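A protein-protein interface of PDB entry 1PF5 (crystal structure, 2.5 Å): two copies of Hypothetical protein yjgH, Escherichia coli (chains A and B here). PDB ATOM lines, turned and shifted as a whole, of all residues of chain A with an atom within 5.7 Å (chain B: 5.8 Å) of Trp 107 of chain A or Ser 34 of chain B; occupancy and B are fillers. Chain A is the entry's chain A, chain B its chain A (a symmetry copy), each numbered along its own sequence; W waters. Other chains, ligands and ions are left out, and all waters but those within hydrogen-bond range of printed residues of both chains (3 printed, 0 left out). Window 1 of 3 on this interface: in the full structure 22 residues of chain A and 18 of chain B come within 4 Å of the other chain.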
ATOM      1  N   PHE A  57     -18.123 -23.713   9.107  1.00  0.00           N
ATOM      2  CA  PHE A  57     -19.034 -23.397  10.201  1.00  0.00           C
ATOM      3  C   PHE A  57     -18.338 -23.563  11.535  1.00  0.00           C
ATOM      4  O   PHE A  57     -18.612 -22.811  12.471  1.00  0.00           O
ATOM      5  CB  PHE A  57     -20.274 -24.277  10.136  1.00  0.00           C
ATOM      6  CG  PHE A  57     -21.339 -23.737   9.232  1.00  0.00           C
ATOM      7  CD1 PHE A  57     -22.129 -22.665   9.637  1.00  0.00           C
ATOM      8  CD2 PHE A  57     -21.542 -24.281   7.969  1.00  0.00           C
ATOM      9  CE1 PHE A  57     -23.106 -22.143   8.797  1.00  0.00           C
ATOM     10  CE2 PHE A  57     -22.519 -23.765   7.118  1.00  0.00           C
ATOM     11  CZ  PHE A  57     -23.303 -22.694   7.534  1.00  0.00           C
ATOM     12  N   VAL A  77     -26.393 -12.708   7.242  1.00  0.00           N
ATOM     13  CA  VAL A  77     -25.614 -13.764   6.607  1.00  0.00           C
ATOM     14  C   VAL A  77     -25.503 -13.625   5.091  1.00  0.00           C
ATOM     15  O   VAL A  77     -26.500 -13.421   4.399  1.00  0.00           O
ATOM     16  CB  VAL A  77     -26.246 -15.141   6.888  1.00  0.00           C
ATOM     17  CG1 VAL A  77     -25.474 -16.222   6.158  1.00  0.00           C
ATOM     18  CG2 VAL A  77     -26.286 -15.407   8.385  1.00  0.00           C
ATOM     19  N   THR A  78     -24.284 -13.736   4.580  1.00  0.00           N
ATOM     20  CA  THR A  78     -24.050 -13.680   3.141  1.00  0.00           C
ATOM     21  C   THR A  78     -23.115 -14.840   2.826  1.00  0.00           C
ATOM     22  O   THR A  78     -22.078 -14.986   3.468  1.00  0.00           O
ATOM     23  CB  THR A  78     -23.347 -12.379   2.702  1.00  0.00           C
ATOM     24  OG1 THR A  78     -24.076 -11.248   3.189  1.00  0.00           O
ATOM     25  CG2 THR A  78     -23.257 -12.314   1.168  1.00  0.00           C
ATOM     26  N   SER A  79     -23.481 -15.672   1.857  1.00  0.00           N
ATOM     27  CA  SER A  79     -22.638 -16.798   1.480  1.00  0.00           C
ATOM     28  C   SER A  79     -22.268 -16.732   0.003  1.00  0.00           C
ATOM     29  O   SER A  79     -23.058 -16.289  -0.838  1.00  0.00           O
ATOM     30  CB  SER A  79     -23.336 -18.125   1.794  1.00  0.00           C
ATOM     31  OG  SER A  79     -24.646 -18.160   1.266  1.00  0.00           O
ATOM     32  N   HIS A  81     -20.509 -18.894  -3.348  1.00  0.00           N
ATOM     33  CA  HIS A  81     -20.350 -20.244  -3.856  1.00  0.00           C
ATOM     34  C   HIS A  81     -19.676 -20.272  -5.214  1.00  0.00           C
ATOM     35  O   HIS A  81     -20.020 -19.493  -6.102  1.00  0.00           O
ATOM     36  CB  HIS A  81     -21.733 -20.878  -3.927  1.00  0.00           C
ATOM     37  CG  HIS A  81     -22.557 -20.616  -2.706  1.00  0.00           C
ATOM     38  ND1 HIS A  81     -22.305 -21.230  -1.497  1.00  0.00           N
ATOM     39  CD2 HIS A  81     -23.542 -19.717  -2.474  1.00  0.00           C
ATOM     40  CE1 HIS A  81     -23.097 -20.717  -0.572  1.00  0.00           C
ATOM     41  NE2 HIS A  81     -23.857 -19.795  -1.138  1.00  0.00           N
ATOM     42  N   ILE A  91     -24.948 -27.958   1.044  1.00  0.00           N
ATOM     43  CA  ILE A  91     -24.987 -26.791   1.913  1.00  0.00           C
ATOM     44  C   ILE A  91     -26.217 -26.783   2.813  1.00  0.00           C
ATOM     45  O   ILE A  91     -26.114 -26.495   4.006  1.00  0.00           O
ATOM     46  CB  ILE A  91     -24.935 -25.497   1.090  1.00  0.00           C
ATOM     47  CG1 ILE A  91     -23.643 -25.472   0.274  1.00  0.00           C
ATOM     48  CG2 ILE A  91     -24.982 -24.296   2.008  1.00  0.00           C
ATOM     49  CD1 ILE A  91     -23.456 -24.240  -0.554  1.00  0.00           C
ATOM     50  N   LYS A  95     -26.657 -26.566   6.745  1.00  0.00           N
ATOM     51  CA  LYS A  95     -27.363 -25.415   7.295  1.00  0.00           C
ATOM     52  C   LYS A  95     -28.545 -25.831   8.166  1.00  0.00           C
ATOM     53  O   LYS A  95     -28.778 -25.232   9.220  1.00  0.00           O
ATOM     54  CB  LYS A  95     -27.861 -24.495   6.172  1.00  0.00           C
ATOM     55  CG  LYS A  95     -28.914 -23.480   6.622  1.00  0.00           C
ATOM     56  CD  LYS A  95     -29.327 -22.553   5.491  1.00  0.00           C
ATOM     57  CE  LYS A  95     -30.563 -21.744   5.843  1.00  0.00           C
ATOM     58  NZ  LYS A  95     -31.764 -22.612   5.938  1.00  0.00           N
ATOM     59  N   PHE A  99     -28.889 -24.541  11.820  1.00  0.00           N
ATOM     60  CA  PHE A  99     -30.030 -23.661  12.028  1.00  0.00           C
ATOM     61  C   PHE A  99     -31.241 -24.562  11.927  1.00  0.00           C
ATOM     62  O   PHE A  99     -31.929 -24.619  10.901  1.00  0.00           O
ATOM     63  CB  PHE A  99     -30.058 -22.583  10.958  1.00  0.00           C
ATOM     64  CG  PHE A  99     -28.866 -21.694  10.998  1.00  0.00           C
ATOM     65  CD1 PHE A  99     -28.619 -20.906  12.117  1.00  0.00           C
ATOM     66  CD2 PHE A  99     -27.962 -21.670   9.944  1.00  0.00           C
ATOM     67  CE1 PHE A  99     -27.483 -20.107  12.188  1.00  0.00           C
ATOM     68  CE2 PHE A  99     -26.824 -20.876  10.002  1.00  0.00           C
ATOM     69  CZ  PHE A  99     -26.582 -20.093  11.126  1.00  0.00           C
ATOM     70  N   PRO A 105     -31.928 -17.351  10.427  1.00  0.00           N
ATOM     71  CA  PRO A 105     -31.233 -16.104  10.104  1.00  0.00           C
ATOM     72  C   PRO A 105     -31.692 -15.644   8.725  1.00  0.00           C
ATOM     73  O   PRO A 105     -32.337 -16.409   8.013  1.00  0.00           O
ATOM     74  CB  PRO A 105     -29.760 -16.522  10.120  1.00  0.00           C
ATOM     75  CG  PRO A 105     -29.815 -17.956   9.649  1.00  0.00           C
ATOM     76  CD  PRO A 105     -31.012 -18.507  10.397  1.00  0.00           C
ATOM     77  N   ASN A 106     -31.402 -14.396   8.358  1.00  0.00           N
ATOM     78  CA  ASN A 106     -31.761 -13.941   7.023  1.00  0.00           C
ATOM     79  C   ASN A 106     -30.697 -14.609   6.152  1.00  0.00           C
ATOM     80  O   ASN A 106     -29.904 -15.407   6.653  1.00  0.00           O
ATOM     81  CB  ASN A 106     -31.685 -12.410   6.899  1.00  0.00           C
ATOM     82  CG  ASN A 106     -30.270 -11.856   7.051  1.00  0.00           C
ATOM     83  OD1 ASN A 106     -29.281 -12.576   6.945  1.00  0.00           O
ATOM     84  ND2 ASN A 106     -30.179 -10.557   7.284  1.00  0.00           N
ATOM     85  N   TRP A 107     -30.655 -14.304   4.864  1.00  0.00           N
ATOM     86  CA  TRP A 107     -29.642 -14.941   4.042  1.00  0.00           C
ATOM     87  C   TRP A 107     -29.562 -14.405   2.622  1.00  0.00           C
ATOM     88  O   TRP A 107     -30.584 -14.114   1.993  1.00  0.00           O
ATOM     89  CB  TRP A 107     -29.893 -16.451   4.001  1.00  0.00           C
ATOM     90  CG  TRP A 107     -28.653 -17.298   3.782  1.00  0.00           C
ATOM     91  CD1 TRP A 107     -27.871 -17.363   2.652  1.00  0.00           C
ATOM     92  CD2 TRP A 107     -28.068 -18.206   4.725  1.00  0.00           C
ATOM     93  NE1 TRP A 107     -26.840 -18.255   2.840  1.00  0.00           N
ATOM     94  CE2 TRP A 107     -26.936 -18.787   4.101  1.00  0.00           C
ATOM     95  CE3 TRP A 107     -28.389 -18.587   6.040  1.00  0.00           C
ATOM     96  CZ2 TRP A 107     -26.124 -19.734   4.751  1.00  0.00           C
ATOM     97  CZ3 TRP A 107     -27.576 -19.531   6.686  1.00  0.00           C
ATOM     98  CH2 TRP A 107     -26.459 -20.090   6.037  1.00  0.00           C
ATOM     99  N   THR A 108     -28.331 -14.271   2.139  1.00  0.00           N
ATOM    100  CA  THR A 108     -28.069 -13.830   0.783  1.00  0.00           C
ATOM    101  C   THR A 108     -26.986 -14.772   0.257  1.00  0.00           C
ATOM    102  O   THR A 108     -25.867 -14.779   0.759  1.00  0.00           O
ATOM    103  CB  THR A 108     -27.578 -12.366   0.732  1.00  0.00           C
ATOM    104  OG1 THR A 108     -28.523 -11.515   1.403  1.00  0.00           O
ATOM    105  CG2 THR A 108     -27.449 -11.913  -0.710  1.00  0.00           C
ATOM    106  N   ALA A 109     -27.343 -15.592  -0.728  1.00  0.00           N
ATOM    107  CA  ALA A 109     -26.418 -16.551  -1.321  1.00  0.00           C
ATOM    108  C   ALA A 109     -26.121 -16.113  -2.742  1.00  0.00           C
ATOM    109  O   ALA A 109     -27.034 -15.882  -3.528  1.00  0.00           O
ATOM    110  CB  ALA A 109     -27.028 -17.941  -1.318  1.00  0.00           C
ATOM    111  N   PHE A 120     -16.672 -22.468  -0.690  1.00  0.00           N
ATOM    112  CA  PHE A 120     -17.753 -21.951   0.116  1.00  0.00           C
ATOM    113  C   PHE A 120     -17.184 -20.948   1.097  1.00  0.00           C
ATOM    114  O   PHE A 120     -16.088 -21.138   1.623  1.00  0.00           O
ATOM    115  CB  PHE A 120     -18.445 -23.108   0.846  1.00  0.00           C
ATOM    116  CG  PHE A 120     -19.377 -22.677   1.949  1.00  0.00           C
ATOM    117  CD1 PHE A 120     -18.893 -22.428   3.231  1.00  0.00           C
ATOM    118  CD2 PHE A 120     -20.737 -22.526   1.708  1.00  0.00           C
ATOM    119  CE1 PHE A 120     -19.749 -22.039   4.256  1.00  0.00           C
ATOM    120  CE2 PHE A 120     -21.601 -22.136   2.732  1.00  0.00           C
ATOM    121  CZ  PHE A 120     -21.103 -21.894   4.003  1.00  0.00           C
ATOM    122  N   ILE A 122     -18.676 -17.852   4.111  1.00  0.00           N
ATOM    123  CA  ILE A 122     -19.806 -17.247   4.794  1.00  0.00           C
ATOM    124  C   ILE A 122     -19.384 -16.003   5.577  1.00  0.00           C
ATOM    125  O   ILE A 122     -18.577 -16.073   6.510  1.00  0.00           O
ATOM    126  CB  ILE A 122     -20.520 -18.296   5.717  1.00  0.00           C
ATOM    127  CG1 ILE A 122     -21.755 -17.669   6.372  1.00  0.00           C
ATOM    128  CG2 ILE A 122     -19.556 -18.834   6.759  1.00  0.00           C
ATOM    129  CD1 ILE A 122     -22.723 -18.677   6.968  1.00  0.00           C
ATOM    130  N   TYR B  16     -39.170 -18.564   1.936  1.00  0.00           N
ATOM    131  CA  TYR B  16     -38.604 -18.362   3.256  1.00  0.00           C
ATOM    132  C   TYR B  16     -38.904 -19.596   4.069  1.00  0.00           C
ATOM    133  O   TYR B  16     -38.103 -20.008   4.901  1.00  0.00           O
ATOM    134  CB  TYR B  16     -39.222 -17.133   3.930  1.00  0.00           C
ATOM    135  CG  TYR B  16     -38.898 -15.833   3.237  1.00  0.00           C
ATOM    136  CD1 TYR B  16     -37.574 -15.445   3.022  1.00  0.00           C
ATOM    137  CD2 TYR B  16     -39.909 -14.987   2.789  1.00  0.00           C
ATOM    138  CE1 TYR B  16     -37.266 -14.246   2.375  1.00  0.00           C
ATOM    139  CE2 TYR B  16     -39.609 -13.786   2.141  1.00  0.00           C
ATOM    140  CZ  TYR B  16     -38.286 -13.424   1.939  1.00  0.00           C
ATOM    141  OH  TYR B  16     -37.990 -12.243   1.301  1.00  0.00           O
ATOM    142  N   TYR B  21     -35.329 -19.414   6.004  1.00  0.00           N
ATOM    143  CA  TYR B  21     -34.548 -18.221   6.302  1.00  0.00           C
ATOM    144  C   TYR B  21     -35.528 -17.062   6.418  1.00  0.00           C
ATOM    145  O   TYR B  21     -36.602 -17.087   5.824  1.00  0.00           O
ATOM    146  CB  TYR B  21     -33.497 -17.939   5.212  1.00  0.00           C
ATOM    147  CG  TYR B  21     -34.021 -17.422   3.887  1.00  0.00           C
ATOM    148  CD1 TYR B  21     -34.830 -18.214   3.075  1.00  0.00           C
ATOM    149  CD2 TYR B  21     -33.672 -16.150   3.426  1.00  0.00           C
ATOM    150  CE1 TYR B  21     -35.282 -17.755   1.832  1.00  0.00           C
ATOM    151  CE2 TYR B  21     -34.119 -15.681   2.187  1.00  0.00           C
ATOM    152  CZ  TYR B  21     -34.922 -16.492   1.398  1.00  0.00           C
ATOM    153  OH  TYR B  21     -35.370 -16.052   0.174  1.00  0.00           O
ATOM    154  N   SER B  22     -35.171 -16.054   7.198  1.00  0.00           N
ATOM    155  CA  SER B  22     -36.046 -14.909   7.386  1.00  0.00           C
ATOM    156  C   SER B  22     -35.850 -13.858   6.304  1.00  0.00           C
ATOM    157  O   SER B  22     -34.746 -13.693   5.774  1.00  0.00           O
ATOM    158  CB  SER B  22     -35.795 -14.284   8.756  1.00  0.00           C
ATOM    159  OG  SER B  22     -36.056 -15.211   9.793  1.00  0.00           O
ATOM    160  N   ALA B  23     -36.931 -13.146   5.986  1.00  0.00           N
ATOM    161  CA  ALA B  23     -36.903 -12.090   4.976  1.00  0.00           C
ATOM    162  C   ALA B  23     -36.011 -10.927   5.439  1.00  0.00           C
ATOM    163  O   ALA B  23     -35.334 -10.293   4.631  1.00  0.00           O
ATOM    164  CB  ALA B  23     -38.330 -11.590   4.696  1.00  0.00           C
ATOM    165  N   ALA B  24     -36.015 -10.657   6.743  1.00  0.00           N
ATOM    166  CA  ALA B  24     -35.215  -9.585   7.317  1.00  0.00           C
ATOM    167  C   ALA B  24     -35.034  -9.849   8.793  1.00  0.00           C
ATOM    168  O   ALA B  24     -35.787 -10.623   9.383  1.00  0.00           O
ATOM    169  CB  ALA B  24     -35.907  -8.243   7.122  1.00  0.00           C
ATOM    170  N   PHE B  32     -31.586  -5.800   8.799  1.00  0.00           N
ATOM    171  CA  PHE B  32     -30.785  -6.449   7.762  1.00  0.00           C
ATOM    172  C   PHE B  32     -31.719  -7.308   6.924  1.00  0.00           C
ATOM    173  O   PHE B  32     -32.226  -8.325   7.394  1.00  0.00           O
ATOM    174  CB  PHE B  32     -29.691  -7.322   8.368  1.00  0.00           C
ATOM    175  CG  PHE B  32     -28.674  -6.556   9.142  1.00  0.00           C
ATOM    176  CD1 PHE B  32     -28.900  -6.226  10.477  1.00  0.00           C
ATOM    177  CD2 PHE B  32     -27.492  -6.139   8.535  1.00  0.00           C
ATOM    178  CE1 PHE B  32     -27.957  -5.486  11.200  1.00  0.00           C
ATOM    179  CE2 PHE B  32     -26.547  -5.401   9.243  1.00  0.00           C
ATOM    180  CZ  PHE B  32     -26.779  -5.073  10.580  1.00  0.00           C
ATOM    181  N   VAL B  33     -31.935  -6.887   5.683  1.00  0.00           N
ATOM    182  CA  VAL B  33     -32.829  -7.579   4.766  1.00  0.00           C
ATOM    183  C   VAL B  33     -32.120  -8.600   3.884  1.00  0.00           C
ATOM    184  O   VAL B  33     -31.037  -8.340   3.370  1.00  0.00           O
ATOM    185  CB  VAL B  33     -33.545  -6.560   3.850  1.00  0.00           C
ATOM    186  CG1 VAL B  33     -34.665  -7.237   3.080  1.00  0.00           C
ATOM    187  CG2 VAL B  33     -34.070  -5.401   4.685  1.00  0.00           C
ATOM    188  N   SER B  34     -32.733  -9.768   3.718  1.00  0.00           N
ATOM    189  CA  SER B  34     -32.168 -10.801   2.858  1.00  0.00           C
ATOM    190  C   SER B  34     -32.225 -10.229   1.450  1.00  0.00           C
ATOM    191  O   SER B  34     -33.023  -9.334   1.170  1.00  0.00           O
ATOM    192  CB  SER B  34     -33.012 -12.085   2.908  1.00  0.00           C
ATOM    193  OG  SER B  34     -33.066 -12.633   4.213  1.00  0.00           O
ATOM    194  N   GLY B  35     -31.378 -10.724   0.561  1.00  0.00           N
ATOM    195  CA  GLY B  35     -31.427 -10.227  -0.795  1.00  0.00           C
ATOM    196  C   GLY B  35     -32.831 -10.466  -1.317  1.00  0.00           C
ATOM    197  O   GLY B  35     -33.407 -11.531  -1.100  1.00  0.00           O
ATOM    198  N   GLN B  36     -33.394  -9.469  -1.989  1.00  0.00           N
ATOM    199  CA  GLN B  36     -34.728  -9.588  -2.553  1.00  0.00           C
ATOM    200  C   GLN B  36     -34.624  -9.837  -4.060  1.00  0.00           C
ATOM    201  O   GLN B  36     -33.748  -9.288  -4.737  1.00  0.00           O
ATOM    202  CB  GLN B  36     -35.531  -8.312  -2.276  1.00  0.00           C
ATOM    203  CG  GLN B  36     -35.769  -8.044  -0.797  1.00  0.00           C
ATOM    204  CD  GLN B  36     -36.586  -9.135  -0.118  1.00  0.00           C
ATOM    205  OE1 GLN B  36     -37.734  -9.391  -0.484  1.00  0.00           O
ATOM    206  NE2 GLN B  36     -35.992  -9.783   0.877  1.00  0.00           N
ATOM    207  N   LEU B  60     -39.175  -6.111  -2.003  1.00  0.00           N
ATOM    208  CA  LEU B  60     -38.337  -5.402  -1.041  1.00  0.00           C
ATOM    209  C   LEU B  60     -39.189  -4.461  -0.197  1.00  0.00           C
ATOM    210  O   LEU B  60     -39.111  -4.468   1.035  1.00  0.00           O
ATOM    211  CB  LEU B  60     -37.254  -4.588  -1.757  1.00  0.00           C
ATOM    212  CG  LEU B  60     -36.418  -3.647  -0.870  1.00  0.00           C
ATOM    213  CD1 LEU B  60     -35.749  -4.411   0.259  1.00  0.00           C
ATOM    214  CD2 LEU B  60     -35.375  -2.957  -1.717  1.00  0.00           C
ATOM    215  N   GLU B 121     -30.725  -9.187  -7.882  1.00  0.00           N
ATOM    216  CA  GLU B 121     -30.937  -9.328  -6.451  1.00  0.00           C
ATOM    217  C   GLU B 121     -30.429  -8.078  -5.778  1.00  0.00           C
ATOM    218  O   GLU B 121     -29.420  -7.509  -6.198  1.00  0.00           O
ATOM    219  CB  GLU B 121     -30.195 -10.552  -5.910  1.00  0.00           C
ATOM    220  CG  GLU B 121     -30.374 -10.779  -4.412  1.00  0.00           C
ATOM    221  CD  GLU B 121     -30.218 -12.240  -4.015  1.00  0.00           C
ATOM    222  OE1 GLU B 121     -30.008 -12.518  -2.808  1.00  0.00           O
ATOM    223  OE2 GLU B 121     -30.313 -13.112  -4.909  1.00  0.00           O
ATOM    224  N   ILE B 122     -31.140  -7.646  -4.741  1.00  0.00           N
ATOM    225  CA  ILE B 122     -30.768  -6.443  -4.017  1.00  0.00           C
ATOM    226  C   ILE B 122     -30.760  -6.681  -2.506  1.00  0.00           C
ATOM    227  O   ILE B 122     -31.790  -6.992  -1.899  1.00  0.00           O
ATOM    228  CB  ILE B 122     -31.707  -5.249  -4.408  1.00  0.00           C
ATOM    229  CG1 ILE B 122     -31.257  -3.968  -3.699  1.00  0.00           C
ATOM    230  CG2 ILE B 122     -33.153  -5.580  -4.088  1.00  0.00           C
ATOM    231  CD1 ILE B 122     -31.838  -2.694  -4.286  1.00  0.00           C
ATOM    232  N   LYS B 123     -29.566  -6.564  -1.920  1.00  0.00           N
ATOM    233  CA  LYS B 123     -29.356  -6.747  -0.490  1.00  0.00           C
ATOM    234  C   LYS B 123     -29.327  -5.354   0.119  1.00  0.00           C
ATOM    235  O   LYS B 123     -28.552  -4.495  -0.299  1.00  0.00           O
ATOM    236  CB  LYS B 123     -28.033  -7.473  -0.235  1.00  0.00           C
ATOM    237  CG  LYS B 123     -27.817  -7.846   1.221  1.00  0.00           C
ATOM    238  CD  LYS B 123     -26.490  -8.566   1.431  1.00  0.00           C
ATOM    239  CE  LYS B 123     -26.217  -8.774   2.916  1.00  0.00           C
ATOM    240  NZ  LYS B 123     -26.100  -7.465   3.640  1.00  0.00           N
ATOM    241  N   VAL B 124     -30.157  -5.145   1.130  1.00  0.00           N
ATOM    242  CA  VAL B 124     -30.290  -3.838   1.753  1.00  0.00           C
ATOM    243  C   VAL B 124     -30.208  -3.808   3.286  1.00  0.00           C
ATOM    244  O   VAL B 124     -30.506  -4.796   3.960  1.00  0.00           O
ATOM    245  CB  VAL B 124     -31.646  -3.236   1.278  1.00  0.00           C
ATOM    246  CG1 VAL B 124     -32.277  -2.384   2.351  1.00  0.00           C
ATOM    247  CG2 VAL B 124     -31.433  -2.451  -0.007  1.00  0.00           C
HETATM  248  O   HOH W   1     -30.180 -15.159  -1.749  1.00  0.00           O
HETATM  249  O   HOH W   2     -29.590 -15.775  -4.555  1.00  0.00           O
HETATM  250  O   HOH W   3     -32.067 -14.275  -0.172  1.00  0.00           O
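The backbone carbonyl oxygen (O) of Pro 105 of chain A lies within hydrogen-bond range of the backbone NH (N) of Ser 22 of chain B (3.0 Å). The backbone carbonyl oxygen (O) of Phe 32 of chain B is in hydrogen-bond range of the side-chain amide nitrogen (ND2) of Asn 106 of chain A (3.0 Å). The backbone NH (N) of Trp 107 of chain A is in hydrogen-bond range of the side-chain hydroxyl (OG) of Ser 34 of chain B (3.0 Å). OG1 of Thr 108 of chain A lies within hydrogen-bond range of N of Gly 35 of chain B, 3.1 Å away.
The backbone NH (N) of Val 77 of chain A is in hydrogen-bond range of the side-chain amide oxygen (OD1) of Asn 106 of chain A (2.9 Å). The backbone carbonyl oxygen of Val 77 of chain A sits at hydrogen-bond distance from the backbone NH of Thr 108 of chain A, at 3.0 Å. The side-chain hydroxyl (OG) of Ser 79 of chain A sits at hydrogen-bond distance from the indole nitrogen (NE1) of Trp 107 of chain A. The backbone carbonyl oxygen of Thr 108 of chain A sits at hydrogen-bond distance from the backbone NH of Ser 79 of chain A (2.8 Å). N of Ser 34 of chain B is in hydrogen-bond range of O of Ala 23 of chain B, 2.8 Å away. The backbone carbonyl oxygen (O) of Ser 34 of chain B sits at hydrogen-bond distance from the side-chain amide nitrogen (NE2) of Gln 36 of chain B, at 3.0 Å.
Thr 78 of chain A touches Lys 123 of chain B. O of Pro 105 of chain A touches CA of Tyr 21 of chain B (3.3 Å). Ser 22 of chain B touches Asn 106 of chain A (O to CA, 3.2 Å). CB of Asn 106 of chain A touches OG of Ser 34 of chain B, 3.0 Å away. Trp 107 of chain A touches Tyr 21 of chain B. O of Trp 107 of chain A touches N of Gly 35 of chain B (3.8 Å). Ser 34 of chain B touches Thr 108 of chain A (C to OG1, 3.9 Å). Glu 121 of chain B touches Thr 108 of chain A (OE1 to CG2, 3.4 Å). Lys 123 of chain B touches Thr 108 of chain A.
Printed residues of chain B within 4 Å of Thr 108 of chain A: Ser 34 (3.9 Å), Gly 35 (3.1 Å), Glu 121 (3.4 Å) and Lys 123 (3.6 Å). Ser 34 of chain B touches three residues of chain A. Of the printed residues of chain A, Gly 35 of chain B touches Trp 107 (3.8 Å) and Thr 108 (3.1 Å). The nearest residue of chain A that does not touch Ser 34 of chain B is Pro 105 of chain A (5.4 Å). The nearest printed residue of chain A that does not touch Gly 35 of chain B is Ala 109 of chain A (6.5 Å).
Hydrophobic or aromatic side chains of chain B that line the printed part of chain A: Tyr 21 and Phe 32. Along chain A the printed residues that touch a printed residue of chain B span positions 78 to 108.
Position printed for both chains: 122.
Water W3 bridges O of Trp 107 of chain A and O of Gly 35 of chain B. Water W2 lies within hydrogen-bond range of O of Ala 109 of chain A (2.8 Å) and OE2 of Glu 121 of chain B (2.8 Å). Water W1 lies within hydrogen-bond range of OE1 of Glu 121 of chain B (2.9 Å) and N of Ala 109 of chain A (3.0 Å).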
